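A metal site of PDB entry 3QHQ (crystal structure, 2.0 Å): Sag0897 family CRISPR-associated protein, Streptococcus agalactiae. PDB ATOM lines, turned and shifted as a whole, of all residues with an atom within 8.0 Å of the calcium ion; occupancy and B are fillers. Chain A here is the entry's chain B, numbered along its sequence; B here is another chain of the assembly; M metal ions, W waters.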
ATOM      1  N   VAL A  71       7.282 -11.571 -30.000  1.00  0.00           N
ATOM      2  CA  VAL A  71       8.549 -11.851 -30.717  1.00  0.00           C
ATOM      3  C   VAL A  71       8.368 -12.738 -31.949  1.00  0.00           C
ATOM      4  O   VAL A  71       9.346 -13.120 -32.593  1.00  0.00           O
ATOM      5  CB  VAL A  71       9.630 -12.471 -29.791  1.00  0.00           C
ATOM      6  CG1 VAL A  71      10.136 -11.453 -28.769  1.00  0.00           C
ATOM      7  CG2 VAL A  71       9.126 -13.753 -29.136  1.00  0.00           C
ATOM      8  N   ILE A 138       9.805 -18.891 -32.356  1.00  0.00           N
ATOM      9  CA  ILE A 138      10.317 -18.799 -30.991  1.00  0.00           C
ATOM     10  C   ILE A 138       9.318 -19.427 -30.016  1.00  0.00           C
ATOM     11  O   ILE A 138       8.113 -19.131 -30.068  1.00  0.00           O
ATOM     12  CB  ILE A 138      10.633 -17.325 -30.619  1.00  0.00           C
ATOM     13  CG1 ILE A 138      11.712 -16.765 -31.551  1.00  0.00           C
ATOM     14  CG2 ILE A 138      11.103 -17.218 -29.159  1.00  0.00           C
ATOM     15  CD1 ILE A 138      11.923 -15.275 -31.453  1.00  0.00           C
ATOM     16  N   GLU A 139       9.819 -20.318 -29.163  1.00  0.00           N
ATOM     17  CA  GLU A 139       9.002 -20.870 -28.083  1.00  0.00           C
ATOM     18  C   GLU A 139       8.881 -19.789 -27.024  1.00  0.00           C
ATOM     19  O   GLU A 139       9.891 -19.246 -26.578  1.00  0.00           O
ATOM     20  CB  GLU A 139       9.675 -22.119 -27.498  1.00  0.00           C
ATOM     21  CG  GLU A 139       8.781 -22.956 -26.570  1.00  0.00           C
ATOM     22  CD  GLU A 139       8.678 -22.391 -25.147  1.00  0.00           C
ATOM     23  OE1 GLU A 139       9.429 -21.466 -24.799  1.00  0.00           O
ATOM     24  OE2 GLU A 139       7.840 -22.895 -24.379  1.00  0.00           O
ATOM     25  N   THR A 140       7.640 -19.478 -26.624  1.00  0.00           N
ATOM     26  CA  THR A 140       7.407 -18.463 -25.583  1.00  0.00           C
ATOM     27  C   THR A 140       6.534 -18.950 -24.420  1.00  0.00           C
ATOM     28  O   THR A 140       6.525 -18.341 -23.366  1.00  0.00           O
ATOM     29  CB  THR A 140       6.799 -17.146 -26.145  1.00  0.00           C
ATOM     30  OG1 THR A 140       5.537 -17.414 -26.768  1.00  0.00           O
ATOM     31  CG2 THR A 140       7.743 -16.481 -27.145  1.00  0.00           C
ATOM     32  N   GLN A 141       5.805 -20.047 -24.637  1.00  0.00           N
ATOM     33  CA  GLN A 141       4.798 -20.511 -23.673  1.00  0.00           C
ATOM     34  C   GLN A 141       5.374 -20.705 -22.266  1.00  0.00           C
ATOM     35  O   GLN A 141       4.809 -20.213 -21.282  1.00  0.00           O
ATOM     36  CB  GLN A 141       4.158 -21.806 -24.172  1.00  0.00           C
ATOM     37  CG  GLN A 141       2.842 -22.161 -23.498  1.00  0.00           C
ATOM     38  CD  GLN A 141       2.140 -23.330 -24.176  1.00  0.00           C
ATOM     39  OE1 GLN A 141       2.608 -24.470 -24.151  1.00  0.00           O
ATOM     40  NE2 GLN A 141       0.991 -23.044 -24.797  1.00  0.00           N
ATOM     41  N   SER A 142       6.507 -21.401 -22.188  1.00  0.00           N
ATOM     42  CA  SER A 142       7.127 -21.730 -20.905  1.00  0.00           C
ATOM     43  C   SER A 142       8.060 -20.647 -20.345  1.00  0.00           C
ATOM     44  O   SER A 142       8.610 -20.815 -19.246  1.00  0.00           O
ATOM     45  CB  SER A 142       7.887 -23.051 -21.015  1.00  0.00           C
ATOM     46  OG  SER A 142       8.941 -22.929 -21.962  1.00  0.00           O
ATOM     47  N   ASP A 143       8.227 -19.547 -21.086  1.00  0.00           N
ATOM     48  CA  ASP A 143       9.193 -18.491 -20.744  1.00  0.00           C
ATOM     49  C   ASP A 143       9.141 -18.034 -19.298  1.00  0.00           C
ATOM     50  O   ASP A 143       8.071 -17.704 -18.777  1.00  0.00           O
ATOM     51  CB  ASP A 143       8.964 -17.244 -21.605  1.00  0.00           C
ATOM     52  CG  ASP A 143       9.497 -17.396 -23.010  1.00  0.00           C
ATOM     53  OD1 ASP A 143      10.002 -18.483 -23.354  1.00  0.00           O
ATOM     54  OD2 ASP A 143       9.394 -16.411 -23.782  1.00  0.00           O
ATOM     55  N   THR A 144      10.311 -17.982 -18.664  1.00  0.00           N
ATOM     56  CA  THR A 144      10.482 -17.143 -17.486  1.00  0.00           C
ATOM     57  C   THR A 144      10.660 -15.713 -18.022  1.00  0.00           C
ATOM     58  O   THR A 144      10.878 -15.536 -19.215  1.00  0.00           O
ATOM     59  CB  THR A 144      11.728 -17.536 -16.671  1.00  0.00           C
ATOM     60  OG1 THR A 144      12.895 -17.378 -17.486  1.00  0.00           O
ATOM     61  CG2 THR A 144      11.618 -18.982 -16.187  1.00  0.00           C
ATOM     62  N   GLU A 147      14.086 -15.427 -19.546  1.00  0.00           N
ATOM     63  CA  GLU A 147      14.129 -16.097 -20.856  1.00  0.00           C
ATOM     64  C   GLU A 147      13.537 -15.220 -21.958  1.00  0.00           C
ATOM     65  O   GLU A 147      14.109 -15.131 -23.050  1.00  0.00           O
ATOM     66  CB  GLU A 147      13.448 -17.462 -20.797  1.00  0.00           C
ATOM     67  CG  GLU A 147      14.327 -18.572 -20.166  1.00  0.00           C
ATOM     68  CD  GLU A 147      13.586 -19.894 -19.989  1.00  0.00           C
ATOM     69  OE1 GLU A 147      12.339 -19.902 -19.994  1.00  0.00           O
ATOM     70  OE2 GLU A 147      14.258 -20.931 -19.848  1.00  0.00           O
ATOM     71  N   LYS A 148      12.407 -14.586 -21.668  1.00  0.00           N
ATOM     72  CA  LYS A 148      11.741 -13.700 -22.633  1.00  0.00           C
ATOM     73  C   LYS A 148      12.527 -12.422 -22.897  1.00  0.00           C
ATOM     74  O   LYS A 148      12.598 -11.963 -24.037  1.00  0.00           O
ATOM     75  CB  LYS A 148      10.289 -13.394 -22.200  1.00  0.00           C
ATOM     76  CG  LYS A 148       9.526 -12.475 -23.164  1.00  0.00           C
ATOM     77  CD  LYS A 148       9.463 -13.026 -24.604  1.00  0.00           C
ATOM     78  CE  LYS A 148       8.451 -12.268 -25.451  1.00  0.00           C
ATOM     79  NZ  LYS A 148       7.030 -12.375 -24.913  1.00  0.00           N
ATOM     80  N   GLU A 151      15.124 -13.473 -25.344  1.00  0.00           N
ATOM     81  CA  GLU A 151      14.503 -13.618 -26.669  1.00  0.00           C
ATOM     82  C   GLU A 151      14.253 -12.252 -27.337  1.00  0.00           C
ATOM     83  O   GLU A 151      14.460 -12.103 -28.548  1.00  0.00           O
ATOM     84  CB  GLU A 151      13.188 -14.424 -26.560  1.00  0.00           C
ATOM     85  CG  GLU A 151      13.386 -15.930 -26.343  1.00  0.00           C
ATOM     86  CD  GLU A 151      12.171 -16.620 -25.743  1.00  0.00           C
ATOM     87  OE1 GLU A 151      11.147 -15.926 -25.513  1.00  0.00           O
ATOM     88  OE2 GLU A 151      12.227 -17.851 -25.477  1.00  0.00           O
ATOM     89  N   LEU B 118      18.500 -18.808 -30.674  1.00  0.00           N
ATOM     90  CA  LEU B 118      17.126 -18.626 -30.200  1.00  0.00           C
ATOM     91  C   LEU B 118      16.537 -19.944 -29.740  1.00  0.00           C
ATOM     92  O   LEU B 118      16.883 -21.000 -30.257  1.00  0.00           O
ATOM     93  CB  LEU B 118      16.231 -18.032 -31.297  1.00  0.00           C
ATOM     94  CG  LEU B 118      16.263 -16.523 -31.487  1.00  0.00           C
ATOM     95  CD1 LEU B 118      15.751 -16.176 -32.879  1.00  0.00           C
ATOM     96  CD2 LEU B 118      15.450 -15.823 -30.405  1.00  0.00           C
ATOM     97  N   ASP B 119      15.639 -19.868 -28.750  1.00  0.00           N
ATOM     98  CA  ASP B 119      14.885 -21.030 -28.314  1.00  0.00           C
ATOM     99  C   ASP B 119      13.734 -21.255 -29.280  1.00  0.00           C
ATOM    100  O   ASP B 119      12.706 -20.566 -29.236  1.00  0.00           O
ATOM    101  CB  ASP B 119      14.393 -20.844 -26.885  1.00  0.00           C
ATOM    102  CG  ASP B 119      13.554 -22.003 -26.399  1.00  0.00           C
ATOM    103  OD1 ASP B 119      13.855 -23.165 -26.776  1.00  0.00           O
ATOM    104  OD2 ASP B 119      12.591 -21.765 -25.666  1.00  0.00           O
ATOM    105  N   LEU B 120      13.916 -22.220 -30.173  1.00  0.00           N
ATOM    106  CA  LEU B 120      13.004 -22.412 -31.292  1.00  0.00           C
ATOM    107  C   LEU B 120      12.159 -23.671 -31.155  1.00  0.00           C
ATOM    108  O   LEU B 120      12.617 -24.697 -30.642  1.00  0.00           O
ATOM    109  CB  LEU B 120      13.780 -22.428 -32.615  1.00  0.00           C
ATOM    110  CG  LEU B 120      14.530 -21.146 -32.996  1.00  0.00           C
ATOM    111  CD1 LEU B 120      15.382 -21.379 -34.234  1.00  0.00           C
ATOM    112  CD2 LEU B 120      13.557 -19.967 -33.208  1.00  0.00           C
ATOM    113  N   GLU B 121      10.930 -23.561 -31.607  1.00  0.00           N
ATOM    114  CA  GLU B 121      10.012 -24.686 -31.713  1.00  0.00           C
ATOM    115  C   GLU B 121       9.414 -24.703 -33.116  1.00  0.00           C
ATOM    116  O   GLU B 121       9.658 -23.776 -33.910  1.00  0.00           O
ATOM    117  CB  GLU B 121       8.916 -24.603 -30.640  1.00  0.00           C
ATOM    118  CG  GLU B 121       7.940 -23.431 -30.815  1.00  0.00           C
ATOM    119  CD  GLU B 121       6.810 -23.452 -29.807  1.00  0.00           C
ATOM    120  OE1 GLU B 121       6.601 -24.499 -29.155  1.00  0.00           O
ATOM    121  OE2 GLU B 121       6.121 -22.425 -29.658  1.00  0.00           O
HETATM  122 CA    CA M   1      11.316 -19.882 -24.657  1.00  0.00          CA
HETATM  123  O   HOH W   1      13.633 -19.595 -23.729  1.00  0.00           O
HETATM  124  O   HOH W   2      11.391 -21.140 -22.506  1.00  0.00           O
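OE2 of Glu 139 is in hydrogen-bond range of OG of Ser 142 (2.7 Å).
Within 4 Å of the calcium ion: Glu 139, Asp 143, Glu 151 and Asp 119 of chain B.
The calcium ion is bound by OD1 of Asp 143 (2.3 Å), OE2 of Glu 151 (2.4 Å), OE1 of Glu 139 (2.5 Å), O of Glu 139 (2.5 Å), OD2 of Asp 119 of chain B (2.5 Å), water W2 (2.5 Å) and water W1 (2.5 Å).
The calcium ion has seven donor atoms within binding distance.
Water W2 bridges OE1 of Glu 147 (3.0 Å) and OG of Ser 142 (3.1 Å).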
